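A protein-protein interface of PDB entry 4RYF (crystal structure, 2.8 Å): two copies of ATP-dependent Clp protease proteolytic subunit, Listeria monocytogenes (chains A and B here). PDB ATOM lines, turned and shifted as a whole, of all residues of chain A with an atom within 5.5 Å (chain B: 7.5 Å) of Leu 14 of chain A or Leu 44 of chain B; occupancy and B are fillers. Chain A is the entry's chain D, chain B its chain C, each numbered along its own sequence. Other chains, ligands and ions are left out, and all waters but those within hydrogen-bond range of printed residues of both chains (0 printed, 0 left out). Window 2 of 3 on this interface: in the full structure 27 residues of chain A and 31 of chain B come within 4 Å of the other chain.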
ATOM      1  N   ILE A  10      -3.172 -20.097 -12.794  1.00  0.00           N
ATOM      2  CA  ILE A  10      -2.342 -18.859 -12.669  1.00  0.00           C
ATOM      3  C   ILE A  10      -2.802 -17.987 -11.490  1.00  0.00           C
ATOM      4  O   ILE A  10      -2.040 -17.154 -10.993  1.00  0.00           O
ATOM      5  CB  ILE A  10      -2.260 -18.086 -14.016  1.00  0.00           C
ATOM      6  CG1 ILE A  10      -1.392 -18.857 -15.030  1.00  0.00           C
ATOM      7  CG2 ILE A  10      -1.741 -16.662 -13.833  1.00  0.00           C
ATOM      8  CD1 ILE A  10       0.079 -18.990 -14.671  1.00  0.00           C
ATOM      9  N   THR A  11      -4.038 -18.194 -11.034  1.00  0.00           N
ATOM     10  CA  THR A  11      -4.465 -17.671  -9.731  1.00  0.00           C
ATOM     11  C   THR A  11      -3.878 -18.582  -8.644  1.00  0.00           C
ATOM     12  O   THR A  11      -3.944 -18.275  -7.450  1.00  0.00           O
ATOM     13  CB  THR A  11      -6.001 -17.574  -9.589  1.00  0.00           C
ATOM     14  OG1 THR A  11      -6.612 -17.487 -10.882  1.00  0.00           O
ATOM     15  CG2 THR A  11      -6.387 -16.349  -8.763  1.00  0.00           C
ATOM     16  N   ASN A  12      -3.314 -19.707  -9.088  1.00  0.00           N
ATOM     17  CA  ASN A  12      -2.506 -20.597  -8.256  1.00  0.00           C
ATOM     18  C   ASN A  12      -1.268 -19.883  -7.729  1.00  0.00           C
ATOM     19  O   ASN A  12      -1.087 -19.753  -6.521  1.00  0.00           O
ATOM     20  CB  ASN A  12      -2.074 -21.838  -9.052  1.00  0.00           C
ATOM     21  CG  ASN A  12      -3.109 -22.951  -9.034  1.00  0.00           C
ATOM     22  OD1 ASN A  12      -4.129 -22.869  -8.348  1.00  0.00           O
ATOM     23  ND2 ASN A  12      -2.839 -24.009  -9.789  1.00  0.00           N
ATOM     24  N   ILE A  13      -0.431 -19.413  -8.652  1.00  0.00           N
ATOM     25  CA  ILE A  13       0.823 -18.723  -8.330  1.00  0.00           C
ATOM     26  C   ILE A  13       0.591 -17.283  -7.821  1.00  0.00           C
ATOM     27  O   ILE A  13       1.524 -16.625  -7.351  1.00  0.00           O
ATOM     28  CB  ILE A  13       1.818 -18.797  -9.534  1.00  0.00           C
ATOM     29  CG1 ILE A  13       3.141 -18.068  -9.240  1.00  0.00           C
ATOM     30  CG2 ILE A  13       1.164 -18.310 -10.825  1.00  0.00           C
ATOM     31  CD1 ILE A  13       4.269 -18.388 -10.204  1.00  0.00           C
ATOM     32  N   LEU A  14      -0.660 -16.822  -7.877  1.00  0.00           N
ATOM     33  CA  LEU A  14      -1.016 -15.439  -7.522  1.00  0.00           C
ATOM     34  C   LEU A  14      -1.430 -15.195  -6.064  1.00  0.00           C
ATOM     35  O   LEU A  14      -0.860 -14.329  -5.398  1.00  0.00           O
ATOM     36  CB  LEU A  14      -2.083 -14.890  -8.483  1.00  0.00           C
ATOM     37  CG  LEU A  14      -1.706 -13.823  -9.525  1.00  0.00           C
ATOM     38  CD1 LEU A  14      -1.953 -12.426  -8.974  1.00  0.00           C
ATOM     39  CD2 LEU A  14      -0.280 -13.960 -10.048  1.00  0.00           C
ATOM     40  N   THR A  15      -2.426 -15.933  -5.573  1.00  0.00           N
ATOM     41  CA  THR A  15      -2.834 -15.813  -4.166  1.00  0.00           C
ATOM     42  C   THR A  15      -1.868 -16.566  -3.245  1.00  0.00           C
ATOM     43  O   THR A  15      -1.777 -16.269  -2.050  1.00  0.00           O
ATOM     44  CB  THR A  15      -4.297 -16.249  -3.921  1.00  0.00           C
ATOM     45  OG1 THR A  15      -4.571 -17.462  -4.634  1.00  0.00           O
ATOM     46  CG2 THR A  15      -5.266 -15.162  -4.379  1.00  0.00           C
ATOM     47  N   GLN A  16      -1.156 -17.536  -3.820  1.00  0.00           N
ATOM     48  CA  GLN A  16       0.002 -18.171  -3.188  1.00  0.00           C
ATOM     49  C   GLN A  16       1.055 -17.111  -2.871  1.00  0.00           C
ATOM     50  O   GLN A  16       1.686 -17.145  -1.812  1.00  0.00           O
ATOM     51  CB  GLN A  16       0.583 -19.238  -4.128  1.00  0.00           C
ATOM     52  CG  GLN A  16       2.038 -19.631  -3.894  1.00  0.00           C
ATOM     53  CD  GLN A  16       2.203 -20.784  -2.920  1.00  0.00           C
ATOM     54  OE1 GLN A  16       3.047 -20.734  -2.026  1.00  0.00           O
ATOM     55  NE2 GLN A  16       1.405 -21.833  -3.095  1.00  0.00           N
ATOM     56  N   LYS A  17       1.224 -16.173  -3.802  1.00  0.00           N
ATOM     57  CA  LYS A  17       2.171 -15.071  -3.668  1.00  0.00           C
ATOM     58  C   LYS A  17       1.766 -14.112  -2.545  1.00  0.00           C
ATOM     59  O   LYS A  17       2.618 -13.674  -1.770  1.00  0.00           O
ATOM     60  CB  LYS A  17       2.291 -14.319  -4.998  1.00  0.00           C
ATOM     61  CG  LYS A  17       3.712 -13.986  -5.421  1.00  0.00           C
ATOM     62  CD  LYS A  17       4.394 -15.165  -6.097  1.00  0.00           C
ATOM     63  CE  LYS A  17       5.755 -14.768  -6.639  1.00  0.00           C
ATOM     64  NZ  LYS A  17       6.555 -15.945  -7.071  1.00  0.00           N
ATOM     65  N   LEU A  18       0.471 -13.793  -2.466  1.00  0.00           N
ATOM     66  CA  LEU A  18      -0.082 -12.987  -1.369  1.00  0.00           C
ATOM     67  C   LEU A  18       0.173 -13.628  -0.007  1.00  0.00           C
ATOM     68  O   LEU A  18       0.581 -12.955   0.943  1.00  0.00           O
ATOM     69  CB  LEU A  18      -1.595 -12.778  -1.540  1.00  0.00           C
ATOM     70  CG  LEU A  18      -2.212 -11.445  -1.995  1.00  0.00           C
ATOM     71  CD1 LEU A  18      -1.471 -10.231  -1.438  1.00  0.00           C
ATOM     72  CD2 LEU A  18      -2.321 -11.366  -3.510  1.00  0.00           C
ATOM     73  N   THR B  15      -5.843 -12.396 -16.796  1.00  0.00           N
ATOM     74  CA  THR B  15      -5.425 -11.665 -15.589  1.00  0.00           C
ATOM     75  C   THR B  15      -3.900 -11.691 -15.426  1.00  0.00           C
ATOM     76  O   THR B  15      -3.324 -10.834 -14.750  1.00  0.00           O
ATOM     77  CB  THR B  15      -6.132 -12.162 -14.306  1.00  0.00           C
ATOM     78  OG1 THR B  15      -6.161 -13.595 -14.287  1.00  0.00           O
ATOM     79  CG2 THR B  15      -7.559 -11.622 -14.236  1.00  0.00           C
ATOM     80  N   GLN B  16      -3.268 -12.682 -16.057  1.00  0.00           N
ATOM     81  CA  GLN B  16      -1.818 -12.719 -16.257  1.00  0.00           C
ATOM     82  C   GLN B  16      -1.379 -11.484 -17.040  1.00  0.00           C
ATOM     83  O   GLN B  16      -0.345 -10.882 -16.741  1.00  0.00           O
ATOM     84  CB  GLN B  16      -1.436 -13.998 -17.017  1.00  0.00           C
ATOM     85  CG  GLN B  16      -0.101 -13.975 -17.755  1.00  0.00           C
ATOM     86  CD  GLN B  16       1.064 -14.451 -16.907  1.00  0.00           C
ATOM     87  OE1 GLN B  16       2.125 -13.827 -16.891  1.00  0.00           O
ATOM     88  NE2 GLN B  16       0.877 -15.563 -16.203  1.00  0.00           N
ATOM     89  N   ILE B  19      -1.568  -8.368 -14.840  1.00  0.00           N
ATOM     90  CA  ILE B  19      -0.470  -8.372 -13.879  1.00  0.00           C
ATOM     91  C   ILE B  19       0.886  -8.172 -14.575  1.00  0.00           C
ATOM     92  O   ILE B  19       1.834  -7.667 -13.965  1.00  0.00           O
ATOM     93  CB  ILE B  19      -0.528  -9.642 -12.981  1.00  0.00           C
ATOM     94  CG1 ILE B  19      -0.814  -9.260 -11.522  1.00  0.00           C
ATOM     95  CG2 ILE B  19       0.713 -10.521 -13.124  1.00  0.00           C
ATOM     96  CD1 ILE B  19      -2.194  -8.675 -11.284  1.00  0.00           C
ATOM     97  N   ARG B  22       2.153  -4.488 -14.937  1.00  0.00           N
ATOM     98  CA  ARG B  22       2.727  -3.887 -13.728  1.00  0.00           C
ATOM     99  C   ARG B  22       2.157  -2.479 -13.532  1.00  0.00           C
ATOM    100  O   ARG B  22       2.895  -1.526 -13.273  1.00  0.00           O
ATOM    101  CB  ARG B  22       4.263  -3.847 -13.795  1.00  0.00           C
ATOM    102  CG  ARG B  22       4.936  -5.072 -14.406  1.00  0.00           C
ATOM    103  CD  ARG B  22       5.347  -6.099 -13.361  1.00  0.00           C
ATOM    104  NE  ARG B  22       6.297  -5.546 -12.397  1.00  0.00           N
ATOM    105  CZ  ARG B  22       6.560  -6.088 -11.211  1.00  0.00           C
ATOM    106  NH1 ARG B  22       7.433  -5.510 -10.397  1.00  0.00           N
ATOM    107  NH2 ARG B  22       5.946  -7.203 -10.835  1.00  0.00           N
ATOM    108  N   VAL B  38      -4.092  -0.412  -2.906  1.00  0.00           N
ATOM    109  CA  VAL B  38      -2.796  -0.063  -3.482  1.00  0.00           C
ATOM    110  C   VAL B  38      -1.670  -0.844  -2.794  1.00  0.00           C
ATOM    111  O   VAL B  38      -0.823  -1.426  -3.473  1.00  0.00           O
ATOM    112  CB  VAL B  38      -2.547   1.464  -3.453  1.00  0.00           C
ATOM    113  CG1 VAL B  38      -1.157   1.804  -3.971  1.00  0.00           C
ATOM    114  CG2 VAL B  38      -3.598   2.185  -4.284  1.00  0.00           C
ATOM    115  N   SER B  39      -1.684  -0.878  -1.460  1.00  0.00           N
ATOM    116  CA  SER B  39      -0.700  -1.646  -0.692  1.00  0.00           C
ATOM    117  C   SER B  39      -0.657  -3.113  -1.123  1.00  0.00           C
ATOM    118  O   SER B  39       0.421  -3.652  -1.379  1.00  0.00           O
ATOM    119  CB  SER B  39      -0.965  -1.541   0.811  1.00  0.00           C
ATOM    120  OG  SER B  39      -0.648  -0.249   1.292  1.00  0.00           O
ATOM    121  N   LYS B  40      -1.829  -3.744  -1.212  1.00  0.00           N
ATOM    122  CA  LYS B  40      -1.944  -5.124  -1.689  1.00  0.00           C
ATOM    123  C   LYS B  40      -1.344  -5.309  -3.081  1.00  0.00           C
ATOM    124  O   LYS B  40      -0.539  -6.215  -3.294  1.00  0.00           O
ATOM    125  CB  LYS B  40      -3.404  -5.578  -1.688  1.00  0.00           C
ATOM    126  CG  LYS B  40      -3.850  -6.222  -0.390  1.00  0.00           C
ATOM    127  CD  LYS B  40      -5.364  -6.316  -0.324  1.00  0.00           C
ATOM    128  CE  LYS B  40      -5.815  -6.882   1.011  1.00  0.00           C
ATOM    129  NZ  LYS B  40      -7.245  -6.570   1.277  1.00  0.00           N
ATOM    130  N   GLN B  41      -1.735  -4.441  -4.013  1.00  0.00           N
ATOM    131  CA  GLN B  41      -1.256  -4.508  -5.397  1.00  0.00           C
ATOM    132  C   GLN B  41       0.259  -4.329  -5.487  1.00  0.00           C
ATOM    133  O   GLN B  41       0.931  -5.073  -6.204  1.00  0.00           O
ATOM    134  CB  GLN B  41      -1.956  -3.467  -6.273  1.00  0.00           C
ATOM    135  CG  GLN B  41      -3.432  -3.726  -6.514  1.00  0.00           C
ATOM    136  CD  GLN B  41      -4.115  -2.547  -7.175  1.00  0.00           C
ATOM    137  OE1 GLN B  41      -4.018  -2.358  -8.386  1.00  0.00           O
ATOM    138  NE2 GLN B  41      -4.811  -1.748  -6.381  1.00  0.00           N
ATOM    139  N   LEU B  42       0.784  -3.347  -4.756  1.00  0.00           N
ATOM    140  CA  LEU B  42       2.225  -3.088  -4.731  1.00  0.00           C
ATOM    141  C   LEU B  42       3.007  -4.258  -4.136  1.00  0.00           C
ATOM    142  O   LEU B  42       4.010  -4.689  -4.710  1.00  0.00           O
ATOM    143  CB  LEU B  42       2.544  -1.786  -3.987  1.00  0.00           C
ATOM    144  CG  LEU B  42       2.113  -0.467  -4.635  1.00  0.00           C
ATOM    145  CD1 LEU B  42       2.526   0.708  -3.763  1.00  0.00           C
ATOM    146  CD2 LEU B  42       2.671  -0.313  -6.045  1.00  0.00           C
ATOM    147  N   LEU B  43       2.539  -4.776  -3.001  1.00  0.00           N
ATOM    148  CA  LEU B  43       3.163  -5.942  -2.374  1.00  0.00           C
ATOM    149  C   LEU B  43       3.089  -7.182  -3.263  1.00  0.00           C
ATOM    150  O   LEU B  43       4.039  -7.966  -3.323  1.00  0.00           O
ATOM    151  CB  LEU B  43       2.541  -6.232  -1.005  1.00  0.00           C
ATOM    152  CG  LEU B  43       2.864  -5.266   0.137  1.00  0.00           C
ATOM    153  CD1 LEU B  43       2.035  -5.609   1.361  1.00  0.00           C
ATOM    154  CD2 LEU B  43       4.349  -5.270   0.472  1.00  0.00           C
ATOM    155  N   LEU B  44       1.962  -7.347  -3.956  1.00  0.00           N
ATOM    156  CA  LEU B  44       1.780  -8.452  -4.890  1.00  0.00           C
ATOM    157  C   LEU B  44       2.765  -8.353  -6.054  1.00  0.00           C
ATOM    158  O   LEU B  44       3.461  -9.323  -6.363  1.00  0.00           O
ATOM    159  CB  LEU B  44       0.328  -8.500  -5.390  1.00  0.00           C
ATOM    160  CG  LEU B  44      -0.223  -9.665  -6.231  1.00  0.00           C
ATOM    161  CD1 LEU B  44      -0.237  -9.319  -7.713  1.00  0.00           C
ATOM    162  CD2 LEU B  44       0.490 -10.992  -5.978  1.00  0.00           C
ATOM    163  N   LEU B  45       2.831  -7.178  -6.679  1.00  0.00           N
ATOM    164  CA  LEU B  45       3.732  -6.941  -7.810  1.00  0.00           C
ATOM    165  C   LEU B  45       5.208  -7.080  -7.432  1.00  0.00           C
ATOM    166  O   LEU B  45       6.013  -7.564  -8.230  1.00  0.00           O
ATOM    167  CB  LEU B  45       3.467  -5.573  -8.448  1.00  0.00           C
ATOM    168  CG  LEU B  45       2.163  -5.387  -9.237  1.00  0.00           C
ATOM    169  CD1 LEU B  45       1.971  -3.928  -9.617  1.00  0.00           C
ATOM    170  CD2 LEU B  45       2.113  -6.274 -10.475  1.00  0.00           C
ATOM    171  N   GLU B  46       5.552  -6.659  -6.218  1.00  0.00           N
ATOM    172  CA  GLU B  46       6.926  -6.747  -5.725  1.00  0.00           C
ATOM    173  C   GLU B  46       7.410  -8.192  -5.596  1.00  0.00           C
ATOM    174  O   GLU B  46       8.550  -8.501  -5.949  1.00  0.00           O
ATOM    175  CB  GLU B  46       7.066  -6.027  -4.381  1.00  0.00           C
ATOM    176  CG  GLU B  46       8.487  -6.003  -3.831  1.00  0.00           C
ATOM    177  CD  GLU B  46       8.544  -5.710  -2.345  1.00  0.00           C
ATOM    178  OE1 GLU B  46       7.570  -6.036  -1.634  1.00  0.00           O
ATOM    179  OE2 GLU B  46       9.569  -5.160  -1.886  1.00  0.00           O
ATOM    180  N   SER B  47       6.543  -9.069  -5.093  1.00  0.00           N
ATOM    181  CA  SER B  47       6.898 -10.475  -4.897  1.00  0.00           C
ATOM    182  C   SER B  47       6.989 -11.239  -6.217  1.00  0.00           C
ATOM    183  O   SER B  47       7.649 -12.276  -6.288  1.00  0.00           O
ATOM    184  CB  SER B  47       5.920 -11.162  -3.939  1.00  0.00           C
ATOM    185  OG  SER B  47       4.620 -11.222  -4.491  1.00  0.00           O
ATOM    186  N   ILE B  48       6.333 -10.724  -7.257  1.00  0.00           N
ATOM    187  CA  ILE B  48       6.415 -11.323  -8.591  1.00  0.00           C
ATOM    188  C   ILE B  48       7.784 -11.065  -9.229  1.00  0.00           C
ATOM    189  O   ILE B  48       8.454 -12.008  -9.649  1.00  0.00           O
ATOM    190  CB  ILE B  48       5.253 -10.872  -9.512  1.00  0.00           C
ATOM    191  CG1 ILE B  48       3.937 -11.508  -9.047  1.00  0.00           C
ATOM    192  CG2 ILE B  48       5.532 -11.244 -10.966  1.00  0.00           C
ATOM    193  CD1 ILE B  48       2.698 -11.017  -9.770  1.00  0.00           C
ATOM    194  N   SER B  49       8.193  -9.796  -9.289  1.00  0.00           N
ATOM    195  CA  SER B  49       9.506  -9.422  -9.832  1.00  0.00           C
ATOM    196  C   SER B  49       9.970  -8.045  -9.348  1.00  0.00           C
ATOM    197  O   SER B  49       9.260  -7.365  -8.603  1.00  0.00           O
ATOM    198  CB  SER B  49       9.499  -9.471 -11.368  1.00  0.00           C
ATOM    199  OG  SER B  49       8.990  -8.271 -11.924  1.00  0.00           O
ATOM    200  N   ILE B  53       7.178  -0.493 -11.880  1.00  0.00           N
ATOM    201  CA  ILE B  53       5.723  -0.420 -11.759  1.00  0.00           C
ATOM    202  C   ILE B  53       5.268   0.975 -12.183  1.00  0.00           C
ATOM    203  O   ILE B  53       5.891   1.973 -11.818  1.00  0.00           O
ATOM    204  CB  ILE B  53       5.264  -0.718 -10.312  1.00  0.00           C
ATOM    205  CG1 ILE B  53       5.583  -2.171  -9.940  1.00  0.00           C
ATOM    206  CG2 ILE B  53       3.773  -0.439 -10.137  1.00  0.00           C
ATOM    207  CD1 ILE B  53       5.636  -2.432  -8.450  1.00  0.00           C
ATOM    208  N   ILE B  77       8.889  -0.557  -1.217  1.00  0.00           N
ATOM    209  CA  ILE B  77       9.099  -1.715  -2.092  1.00  0.00           C
ATOM    210  C   ILE B  77      10.348  -1.559  -2.967  1.00  0.00           C
ATOM    211  O   ILE B  77      10.764  -0.436  -3.273  1.00  0.00           O
ATOM    212  CB  ILE B  77       7.855  -2.027  -2.964  1.00  0.00           C
ATOM    213  CG1 ILE B  77       7.478  -0.825  -3.840  1.00  0.00           C
ATOM    214  CG2 ILE B  77       6.691  -2.473  -2.086  1.00  0.00           C
ATOM    215  CD1 ILE B  77       6.454  -1.126  -4.914  1.00  0.00           C
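Among the printed residues, merely in contact across the chains: Lys 17 of chain A with Ser 47 of chain B, Leu 14 of chain A with Leu 44 of chain B, Ile 10 of chain A with Gln 16 of chain B, Leu 18 of chain A with Leu 44 of chain B and Lys 17 of chain A with Leu 44 of chain B.
Of the 9 printed residues of chain A, 4 touch a printed residue of chain B. Hydrophobic or aromatic side chains of chain A that line the printed part of chain B: Ile 10, Leu 14 and Leu 18. Along chain B the printed residues that touch a printed residue of chain A span positions 16 to 47. Among the printed residues, no Asp or Glu carboxylate lies within 4 Å of a Lys or Arg side-chain nitrogen of the other chain.
2 positions are printed for both chains. Of the 5 pairs that touch across the chains among the printed residues, none has its exchanged pair printed and touching as well.
Leu 14 of chain A touches just one residue of chain B: Leu 44. Printed residues of chain B within 4 Å of Lys 17 of chain A: Leu 44 and Ser 47. Printed residues of chain B within 4 Å of Leu 18 of chain A: Leu 44 (3.8 Å). Arg 22 of chain B touches none of the printed residues of chain A. Leu 43 of chain B touches none of the printed residues of chain A. Of chain A, only Leu 14 (3.6 Å), Lys 17 (3.9 Å) and Leu 18 (3.8 Å) come within 4 Å of Leu 44 of chain B. Of the printed residues of chain A, Ser 47 of chain B touches Lys 17 (3.1 Å). The nearest printed residue of chain A that does not touch Leu 44 of chain B is Thr 15 of chain A (5.8 Å). The nearest printed residue of chain B that does not touch Lys 17 of chain A is Ile 48 of chain B (4.01 Å).
OG of Ser 47 of chain B is in hydrogen-bond range of O of Leu 44 of chain B, 2.9 Å away.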
